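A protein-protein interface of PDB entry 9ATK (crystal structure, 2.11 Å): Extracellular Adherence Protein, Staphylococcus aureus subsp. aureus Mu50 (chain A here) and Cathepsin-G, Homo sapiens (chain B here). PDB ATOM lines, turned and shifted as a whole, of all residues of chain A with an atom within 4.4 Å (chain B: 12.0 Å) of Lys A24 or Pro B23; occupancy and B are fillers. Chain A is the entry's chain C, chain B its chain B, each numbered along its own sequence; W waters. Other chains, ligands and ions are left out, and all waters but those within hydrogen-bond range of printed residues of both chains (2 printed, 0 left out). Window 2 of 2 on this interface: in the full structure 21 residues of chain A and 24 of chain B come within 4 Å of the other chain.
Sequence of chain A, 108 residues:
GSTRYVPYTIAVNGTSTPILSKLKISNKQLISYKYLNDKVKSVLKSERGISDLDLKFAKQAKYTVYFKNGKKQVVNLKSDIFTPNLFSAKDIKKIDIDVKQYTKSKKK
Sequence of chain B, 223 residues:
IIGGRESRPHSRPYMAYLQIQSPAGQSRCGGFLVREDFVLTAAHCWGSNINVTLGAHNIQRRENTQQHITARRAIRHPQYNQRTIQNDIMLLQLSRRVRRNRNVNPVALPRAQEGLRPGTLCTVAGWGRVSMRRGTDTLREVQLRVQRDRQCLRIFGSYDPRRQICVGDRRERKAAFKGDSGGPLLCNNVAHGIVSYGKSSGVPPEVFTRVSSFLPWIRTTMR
NE2 of Gln B21 sits at hydrogen-bond distance from OH of Tyr A5 (3.0 Å). The backbone NH (N) of Lys A22 is in hydrogen-bond range of the backbone carbonyl oxygen (O) of Gln B26 (2.8 Å). The backbone NH of Lys A24 lies within hydrogen-bond range of the backbone carbonyl oxygen of Ala B24 (2.9 Å).
O of Lys A24 is in hydrogen-bond range of NZ of Lys A39 (2.9 Å). The backbone carbonyl oxygen (O) of Gly B25 is in hydrogen-bond range of the side-chain amide nitrogen (NE2) of Gln B21, at 3.5 Å. NE2 of Gln B26 is in hydrogen-bond range of OE1 of Gln B21 (3.2 Å). The backbone carbonyl oxygen (O) of Gln B21 lies within hydrogen-bond range of the backbone NH (N) of Ser B48. The backbone NH (N) of Gln B21 is in hydrogen-bond range of the backbone carbonyl oxygen (O) of Asn B49 (2.9 Å).
Tyr A5 touches Gln B26 (CZ to NE2, 3.4 Å). Lys A22 touches Gly B25. C of Leu A23 touches O of Ala B24, at 3.8 Å. Lys A24 touches Pro B23 (CE to O, 3.5 Å). CA of Gly B25 touches N of Lys A24, 3.8 Å away.
Pro B23 touches just one residue of chain A: Lys A24 (3.5 Å). No residue of chain B comes within 4 Å of Thr A3. Leu A23 touches just one residue of chain B: Ala B24. Lys A39 touches none of the printed residues of chain B. Printed residues of chain A within 4 Å of Gln B21: Tyr A5 (3.0 Å). Of the printed residues of chain A, Ala B24 touches Leu A23 and Lys A24. Printed residues of chain A within 4 Å of Gln B26: Tyr A5 (3.4 Å) and Lys A22 (2.8 Å). Ile B20 touches none of the printed residues of chain A. The nearest residue of chain B that does not touch Lys A24 is Gln B21 (4.1 Å). The nearest printed residue of chain A that does not touch Pro B23 is Tyr A5 (6.4 Å). The nearest printed residue of chain A that does not touch Gln B21 is Lys A24 (4.1 Å).
Of the 8 printed residues of chain A, 4 touch a printed residue of chain B. Printed residues of chain A that touch a printed residue of chain B: Tyr A5, Lys A22, Leu A23 and Lys A24. Hydrophobic or aromatic side chains of chain A within 4 Å of the printed part of chain B: Tyr A5. Among the printed residues, 8 pairs touch across the chains.
Water W2 lies within hydrogen-bond range of the side-chain amino group of Lys A24 (2.5 Å), the side-chain amide nitrogen of Gln B21 (2.8 Å) and the backbone carbonyl oxygen of Ser B22 (3.0 Å). Water W1 lies within hydrogen-bond range of O of Ala B24 (2.6 Å) and O of Lys A24 (2.7 Å).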
ATOM      1  N   THR A   3     -15.529 -13.462  -8.966  1.00  0.00           N
ATOM      2  CA  THR A   3     -16.445 -12.918  -7.969  1.00  0.00           C
ATOM      3  C   THR A   3     -17.346 -11.831  -8.586  1.00  0.00           C
ATOM      4  O   THR A   3     -18.009 -11.093  -7.848  1.00  0.00           O
ATOM      5  CB  THR A   3     -15.690 -12.322  -6.711  1.00  0.00           C
ATOM      6  OG1 THR A   3     -14.434 -11.737  -7.086  1.00  0.00           O
ATOM      7  CG2 THR A   3     -15.429 -13.385  -5.621  1.00  0.00           C
ATOM      8  N   ARG A   4     -17.371 -11.737  -9.921  1.00  0.00           N
ATOM      9  CA  ARG A   4     -18.236 -10.797 -10.637  1.00  0.00           C
ATOM     10  C   ARG A   4     -18.422 -11.230 -12.098  1.00  0.00           C
ATOM     11  O   ARG A   4     -17.469 -11.682 -12.741  1.00  0.00           O
ATOM     12  CB  ARG A   4     -17.672  -9.370 -10.581  1.00  0.00           C
ATOM     13  CG  ARG A   4     -18.313  -8.486 -11.615  1.00  0.00           C
ATOM     14  CD  ARG A   4     -17.942  -7.036 -11.563  1.00  0.00           C
ATOM     15  NE  ARG A   4     -18.599  -6.386 -12.691  1.00  0.00           N
ATOM     16  CZ  ARG A   4     -19.684  -5.631 -12.591  1.00  0.00           C
ATOM     17  NH1 ARG A   4     -20.151  -5.242 -11.411  1.00  0.00           N
ATOM     18  NH2 ARG A   4     -20.314  -5.259 -13.702  1.00  0.00           N
ATOM     19  N   TYR A   5     -19.642 -11.075 -12.628  1.00  0.00           N
ATOM     20  CA  TYR A   5     -19.996 -11.560 -13.963  1.00  0.00           C
ATOM     21  C   TYR A   5     -20.291 -10.393 -14.887  1.00  0.00           C
ATOM     22  O   TYR A   5     -21.141  -9.553 -14.580  1.00  0.00           O
ATOM     23  CB  TYR A   5     -21.216 -12.486 -13.930  1.00  0.00           C
ATOM     24  CG  TYR A   5     -20.982 -13.775 -13.196  1.00  0.00           C
ATOM     25  CD1 TYR A   5     -20.500 -14.895 -13.858  1.00  0.00           C
ATOM     26  CD2 TYR A   5     -21.226 -13.867 -11.837  1.00  0.00           C
ATOM     27  CE1 TYR A   5     -20.284 -16.087 -13.185  1.00  0.00           C
ATOM     28  CE2 TYR A   5     -21.009 -15.049 -11.148  1.00  0.00           C
ATOM     29  CZ  TYR A   5     -20.545 -16.157 -11.827  1.00  0.00           C
ATOM     30  OH  TYR A   5     -20.332 -17.329 -11.139  1.00  0.00           O
ATOM     31  N   LYS A  22     -22.264 -13.993 -19.762  1.00  0.00           N
ATOM     32  CA  LYS A  22     -21.494 -13.200 -18.813  1.00  0.00           C
ATOM     33  C   LYS A  22     -20.196 -13.925 -18.481  1.00  0.00           C
ATOM     34  O   LYS A  22     -20.211 -15.124 -18.175  1.00  0.00           O
ATOM     35  CB  LYS A  22     -22.276 -12.940 -17.524  1.00  0.00           C
ATOM     36  CG  LYS A  22     -23.409 -11.921 -17.626  1.00  0.00           C
ATOM     37  CD  LYS A  22     -24.121 -11.778 -16.279  1.00  0.00           C
ATOM     38  CE  LYS A  22     -25.434 -11.037 -16.438  1.00  0.00           C
ATOM     39  NZ  LYS A  22     -26.049 -10.685 -15.109  1.00  0.00           N
ATOM     40  N   LEU A  23     -19.087 -13.181 -18.555  1.00  0.00           N
ATOM     41  CA  LEU A  23     -17.760 -13.634 -18.162  1.00  0.00           C
ATOM     42  C   LEU A  23     -17.569 -13.515 -16.660  1.00  0.00           C
ATOM     43  O   LEU A  23     -17.861 -12.469 -16.071  1.00  0.00           O
ATOM     44  CB  LEU A  23     -16.688 -12.764 -18.835  1.00  0.00           C
ATOM     45  CG  LEU A  23     -16.094 -13.075 -20.177  1.00  0.00           C
ATOM     46  CD1 LEU A  23     -14.969 -12.044 -20.472  1.00  0.00           C
ATOM     47  CD2 LEU A  23     -15.574 -14.490 -20.187  1.00  0.00           C
ATOM     48  N   LYS A  24     -17.037 -14.562 -16.038  1.00  0.00           N
ATOM     49  CA  LYS A  24     -16.610 -14.453 -14.648  1.00  0.00           C
ATOM     50  C   LYS A  24     -15.250 -13.760 -14.606  1.00  0.00           C
ATOM     51  O   LYS A  24     -14.300 -14.216 -15.252  1.00  0.00           O
ATOM     52  CB  LYS A  24     -16.525 -15.829 -14.006  1.00  0.00           C
ATOM     53  CG  LYS A  24     -16.202 -15.775 -12.540  1.00  0.00           C
ATOM     54  CD  LYS A  24     -15.919 -17.152 -11.980  1.00  0.00           C
ATOM     55  CE  LYS A  24     -17.116 -18.021 -12.142  1.00  0.00           C
ATOM     56  NZ  LYS A  24     -17.131 -19.084 -11.117  1.00  0.00           N
ATOM     57  N   ILE A  25     -15.147 -12.657 -13.874  1.00  0.00           N
ATOM     58  CA  ILE A  25     -13.860 -11.991 -13.717  1.00  0.00           C
ATOM     59  C   ILE A  25     -13.696 -11.574 -12.264  1.00  0.00           C
ATOM     60  O   ILE A  25     -14.645 -11.113 -11.624  1.00  0.00           O
ATOM     61  CB  ILE A  25     -13.681 -10.786 -14.671  1.00  0.00           C
ATOM     62  CG1 ILE A  25     -14.565  -9.608 -14.292  1.00  0.00           C
ATOM     63  CG2 ILE A  25     -13.925 -11.165 -16.148  1.00  0.00           C
ATOM     64  CD1 ILE A  25     -14.152  -8.345 -15.082  1.00  0.00           C
ATOM     65  N   LYS A  39      -8.846 -13.919 -20.589  1.00  0.00           N
ATOM     66  CA  LYS A  39     -10.251 -14.324 -20.461  1.00  0.00           C
ATOM     67  C   LYS A  39     -10.954 -14.298 -21.804  1.00  0.00           C
ATOM     68  O   LYS A  39     -11.800 -15.153 -22.085  1.00  0.00           O
ATOM     69  CB  LYS A  39     -11.006 -13.418 -19.487  1.00  0.00           C
ATOM     70  CG  LYS A  39     -10.562 -13.543 -18.045  1.00  0.00           C
ATOM     71  CD  LYS A  39     -10.635 -14.989 -17.620  1.00  0.00           C
ATOM     72  CE  LYS A  39     -10.338 -15.151 -16.145  1.00  0.00           C
ATOM     73  NZ  LYS A  39     -11.385 -14.445 -15.370  1.00  0.00           N
ATOM     74  N   GLN B  19     -30.572 -21.907 -17.432  1.00  0.00           N
ATOM     75  CA  GLN B  19     -29.507 -21.182 -16.753  1.00  0.00           C
ATOM     76  C   GLN B  19     -28.290 -22.091 -16.768  1.00  0.00           C
ATOM     77  O   GLN B  19     -28.313 -23.189 -16.188  1.00  0.00           O
ATOM     78  CB  GLN B  19     -29.894 -20.817 -15.319  1.00  0.00           C
ATOM     79  CG  GLN B  19     -31.039 -19.855 -15.219  1.00  0.00           C
ATOM     80  CD  GLN B  19     -31.683 -19.908 -13.858  1.00  0.00           C
ATOM     81  OE1 GLN B  19     -31.398 -19.082 -12.988  1.00  0.00           O
ATOM     82  NE2 GLN B  19     -32.523 -20.912 -13.647  1.00  0.00           N
ATOM     83  N   ILE B  20     -27.248 -21.646 -17.454  1.00  0.00           N
ATOM     84  CA  ILE B  20     -26.071 -22.460 -17.713  1.00  0.00           C
ATOM     85  C   ILE B  20     -24.897 -21.834 -16.977  1.00  0.00           C
ATOM     86  O   ILE B  20     -24.682 -20.620 -17.060  1.00  0.00           O
ATOM     87  CB  ILE B  20     -25.811 -22.566 -19.229  1.00  0.00           C
ATOM     88  CG1 ILE B  20     -27.086 -23.044 -19.943  1.00  0.00           C
ATOM     89  CG2 ILE B  20     -24.633 -23.477 -19.541  1.00  0.00           C
ATOM     90  CD1 ILE B  20     -27.483 -22.181 -21.107  1.00  0.00           C
ATOM     91  N   GLN B  21     -24.132 -22.656 -16.270  1.00  0.00           N
ATOM     92  CA  GLN B  21     -22.926 -22.176 -15.609  1.00  0.00           C
ATOM     93  C   GLN B  21     -21.729 -23.020 -16.038  1.00  0.00           C
ATOM     94  O   GLN B  21     -21.859 -24.216 -16.316  1.00  0.00           O
ATOM     95  CB  GLN B  21     -23.073 -22.197 -14.077  1.00  0.00           C
ATOM     96  CG  GLN B  21     -21.785 -21.811 -13.350  1.00  0.00           C
ATOM     97  CD  GLN B  21     -21.834 -20.423 -12.715  1.00  0.00           C
ATOM     98  OE1 GLN B  21     -22.794 -20.088 -12.013  1.00  0.00           O
ATOM     99  NE2 GLN B  21     -20.794 -19.614 -12.952  1.00  0.00           N
ATOM    100  N   SER B  22     -20.564 -22.382 -16.104  1.00  0.00           N
ATOM    101  CA  SER B  22     -19.290 -23.063 -16.321  1.00  0.00           C
ATOM    102  C   SER B  22     -18.229 -22.336 -15.516  1.00  0.00           C
ATOM    103  O   SER B  22     -18.491 -21.234 -15.019  1.00  0.00           O
ATOM    104  CB  SER B  22     -18.922 -23.085 -17.802  1.00  0.00           C
ATOM    105  OG  SER B  22     -19.664 -24.090 -18.464  1.00  0.00           O
ATOM    106  N   PRO B  23     -17.038 -22.897 -15.346  1.00  0.00           N
ATOM    107  CA  PRO B  23     -15.997 -22.144 -14.627  1.00  0.00           C
ATOM    108  C   PRO B  23     -15.729 -20.779 -15.259  1.00  0.00           C
ATOM    109  O   PRO B  23     -15.335 -19.850 -14.555  1.00  0.00           O
ATOM    110  CB  PRO B  23     -14.780 -23.074 -14.705  1.00  0.00           C
ATOM    111  CG  PRO B  23     -15.404 -24.467 -14.773  1.00  0.00           C
ATOM    112  CD  PRO B  23     -16.672 -24.315 -15.553  1.00  0.00           C
ATOM    113  N   ALA B  24     -16.013 -20.631 -16.560  1.00  0.00           N
ATOM    114  CA  ALA B  24     -15.722 -19.391 -17.276  1.00  0.00           C
ATOM    115  C   ALA B  24     -16.797 -18.314 -17.109  1.00  0.00           C
ATOM    116  O   ALA B  24     -16.479 -17.124 -17.199  1.00  0.00           O
ATOM    117  CB  ALA B  24     -15.530 -19.683 -18.764  1.00  0.00           C
ATOM    118  N   GLY B  25     -18.054 -18.681 -16.876  1.00  0.00           N
ATOM    119  CA  GLY B  25     -19.098 -17.675 -16.747  1.00  0.00           C
ATOM    120  C   GLY B  25     -20.486 -18.300 -16.715  1.00  0.00           C
ATOM    121  O   GLY B  25     -20.638 -19.491 -16.443  1.00  0.00           O
ATOM    122  N   GLN B  26     -21.493 -17.474 -17.005  1.00  0.00           N
ATOM    123  CA  GLN B  26     -22.885 -17.901 -16.956  1.00  0.00           C
ATOM    124  C   GLN B  26     -23.608 -17.494 -18.220  1.00  0.00           C
ATOM    125  O   GLN B  26     -23.311 -16.450 -18.802  1.00  0.00           O
ATOM    126  CB  GLN B  26     -23.665 -17.277 -15.812  1.00  0.00           C
ATOM    127  CG  GLN B  26     -23.372 -17.751 -14.461  1.00  0.00           C
ATOM    128  CD  GLN B  26     -24.047 -16.836 -13.445  1.00  0.00           C
ATOM    129  OE1 GLN B  26     -24.805 -15.933 -13.826  1.00  0.00           O
ATOM    130  NE2 GLN B  26     -23.759 -17.045 -12.165  1.00  0.00           N
ATOM    131  N   SER B  27     -24.615 -18.280 -18.594  1.00  0.00           N
ATOM    132  CA  SER B  27     -25.388 -17.986 -19.784  1.00  0.00           C
ATOM    133  C   SER B  27     -26.856 -18.287 -19.540  1.00  0.00           C
ATOM    134  O   SER B  27     -27.225 -19.131 -18.718  1.00  0.00           O
ATOM    135  CB  SER B  27     -24.891 -18.782 -21.007  1.00  0.00           C
ATOM    136  OG  SER B  27     -23.727 -18.183 -21.580  1.00  0.00           O
ATOM    137  N   ARG B  28     -27.695 -17.592 -20.291  1.00  0.00           N
ATOM    138  CA  ARG B  28     -29.138 -17.801 -20.284  1.00  0.00           C
ATOM    139  C   ARG B  28     -29.545 -18.143 -21.706  1.00  0.00           C
ATOM    140  O   ARG B  28     -29.125 -17.449 -22.646  1.00  0.00           O
ATOM    141  CB  ARG B  28     -29.878 -16.545 -19.799  1.00  0.00           C
ATOM    142  CG  ARG B  28     -30.024 -16.366 -18.269  1.00  0.00           C
ATOM    143  CD  ARG B  28     -28.780 -16.729 -17.475  1.00  0.00           C
ATOM    144  NE  ARG B  28     -28.936 -16.661 -16.017  1.00  0.00           N
ATOM    145  CZ  ARG B  28     -28.179 -17.331 -15.152  1.00  0.00           C
ATOM    146  NH1 ARG B  28     -27.289 -18.233 -15.558  1.00  0.00           N
ATOM    147  NH2 ARG B  28     -28.316 -17.092 -13.847  1.00  0.00           N
ATOM    148  N   CYS B  45     -25.434 -23.564 -26.270  1.00  0.00           N
ATOM    149  CA  CYS B  45     -25.852 -23.302 -24.891  1.00  0.00           C
ATOM    150  C   CYS B  45     -25.242 -24.275 -23.876  1.00  0.00           C
ATOM    151  O   CYS B  45     -25.575 -24.208 -22.690  1.00  0.00           O
ATOM    152  CB  CYS B  45     -27.375 -23.359 -24.779  1.00  0.00           C
ATOM    153  SG  CYS B  45     -28.169 -22.071 -25.774  1.00  0.00           S
ATOM    154  N   TRP B  46     -24.377 -25.181 -24.315  1.00  0.00           N
ATOM    155  CA  TRP B  46     -23.790 -26.167 -23.421  1.00  0.00           C
ATOM    156  C   TRP B  46     -22.939 -25.501 -22.341  1.00  0.00           C
ATOM    157  O   TRP B  46     -22.388 -24.409 -22.528  1.00  0.00           O
ATOM    158  CB  TRP B  46     -22.947 -27.160 -24.221  1.00  0.00           C
ATOM    159  CG  TRP B  46     -22.297 -28.235 -23.417  1.00  0.00           C
ATOM    160  CD1 TRP B  46     -22.824 -29.461 -23.102  1.00  0.00           C
ATOM    161  CD2 TRP B  46     -20.984 -28.200 -22.837  1.00  0.00           C
ATOM    162  NE1 TRP B  46     -21.921 -30.183 -22.357  1.00  0.00           N
ATOM    163  CE2 TRP B  46     -20.784 -29.434 -22.185  1.00  0.00           C
ATOM    164  CE3 TRP B  46     -19.962 -27.246 -22.806  1.00  0.00           C
ATOM    165  CZ2 TRP B  46     -19.607 -29.739 -21.500  1.00  0.00           C
ATOM    166  CZ3 TRP B  46     -18.786 -27.551 -22.125  1.00  0.00           C
ATOM    167  CH2 TRP B  46     -18.624 -28.791 -21.475  1.00  0.00           C
ATOM    168  N   GLY B  47     -22.877 -26.159 -21.184  1.00  0.00           N
ATOM    169  CA  GLY B  47     -22.031 -25.773 -20.063  1.00  0.00           C
ATOM    170  C   GLY B  47     -21.958 -26.930 -19.085  1.00  0.00           C
ATOM    171  O   GLY B  47     -22.507 -28.006 -19.334  1.00  0.00           O
ATOM    172  N   SER B  48     -21.263 -26.690 -17.956  1.00  0.00           N
ATOM    173  CA  SER B  48     -21.018 -27.755 -16.979  1.00  0.00           C
ATOM    174  C   SER B  48     -22.286 -28.132 -16.209  1.00  0.00           C
ATOM    175  O   SER B  48     -22.505 -29.308 -15.906  1.00  0.00           O
ATOM    176  CB  SER B  48     -19.931 -27.353 -15.974  1.00  0.00           C
ATOM    177  OG  SER B  48     -18.798 -26.750 -16.566  1.00  0.00           O
ATOM    178  N   ASN B  49     -23.080 -27.149 -15.803  1.00  0.00           N
ATOM    179  CA  ASN B  49     -24.330 -27.395 -15.101  1.00  0.00           C
ATOM    180  C   ASN B  49     -25.410 -26.565 -15.760  1.00  0.00           C
ATOM    181  O   ASN B  49     -25.196 -25.390 -16.081  1.00  0.00           O
ATOM    182  CB  ASN B  49     -24.258 -27.030 -13.603  1.00  0.00           C
ATOM    183  CG  ASN B  49     -23.043 -27.601 -12.924  1.00  0.00           C
ATOM    184  OD1 ASN B  49     -23.087 -28.718 -12.399  1.00  0.00           O
ATOM    185  ND2 ASN B  49     -21.932 -26.839 -12.924  1.00  0.00           N
ATOM    186  N   ILE B  50     -26.564 -27.178 -15.976  1.00  0.00           N
ATOM    187  CA  ILE B  50     -27.696 -26.493 -16.596  1.00  0.00           C
ATOM    188  C   ILE B  50     -28.900 -26.653 -15.681  1.00  0.00           C
ATOM    189  O   ILE B  50     -29.301 -27.785 -15.355  1.00  0.00           O
ATOM    190  CB  ILE B  50     -28.017 -27.044 -17.992  1.00  0.00           C
ATOM    191  CG1 ILE B  50     -26.761 -27.008 -18.874  1.00  0.00           C
ATOM    192  CG2 ILE B  50     -29.198 -26.307 -18.575  1.00  0.00           C
ATOM    193  CD1 ILE B  50     -27.014 -27.303 -20.370  1.00  0.00           C
ATOM    194  N   ARG B  76     -24.464 -32.439 -26.606  1.00  0.00           N
ATOM    195  CA  ARG B  76     -24.273 -31.777 -27.897  1.00  0.00           C
ATOM    196  C   ARG B  76     -24.220 -32.805 -29.019  1.00  0.00           C
ATOM    197  O   ARG B  76     -23.774 -33.937 -28.823  1.00  0.00           O
ATOM    198  CB  ARG B  76     -22.969 -30.980 -27.916  1.00  0.00           C
ATOM    199  CG  ARG B  76     -22.936 -29.801 -26.966  1.00  0.00           C
ATOM    200  CD  ARG B  76     -21.492 -29.394 -26.678  1.00  0.00           C
ATOM    201  NE  ARG B  76     -20.837 -30.368 -25.817  1.00  0.00           N
ATOM    202  CZ  ARG B  76     -19.553 -30.322 -25.483  1.00  0.00           C
ATOM    203  NH1 ARG B  76     -18.756 -29.364 -25.923  1.00  0.00           N
ATOM    204  NH2 ARG B  76     -19.056 -31.263 -24.690  1.00  0.00           N
HETATM  205  O   HOH W   1     -14.110 -16.145 -17.176  1.00  0.00           O
HETATM  206  O   HOH W   2     -18.525 -20.907 -12.031  1.00  0.00           O
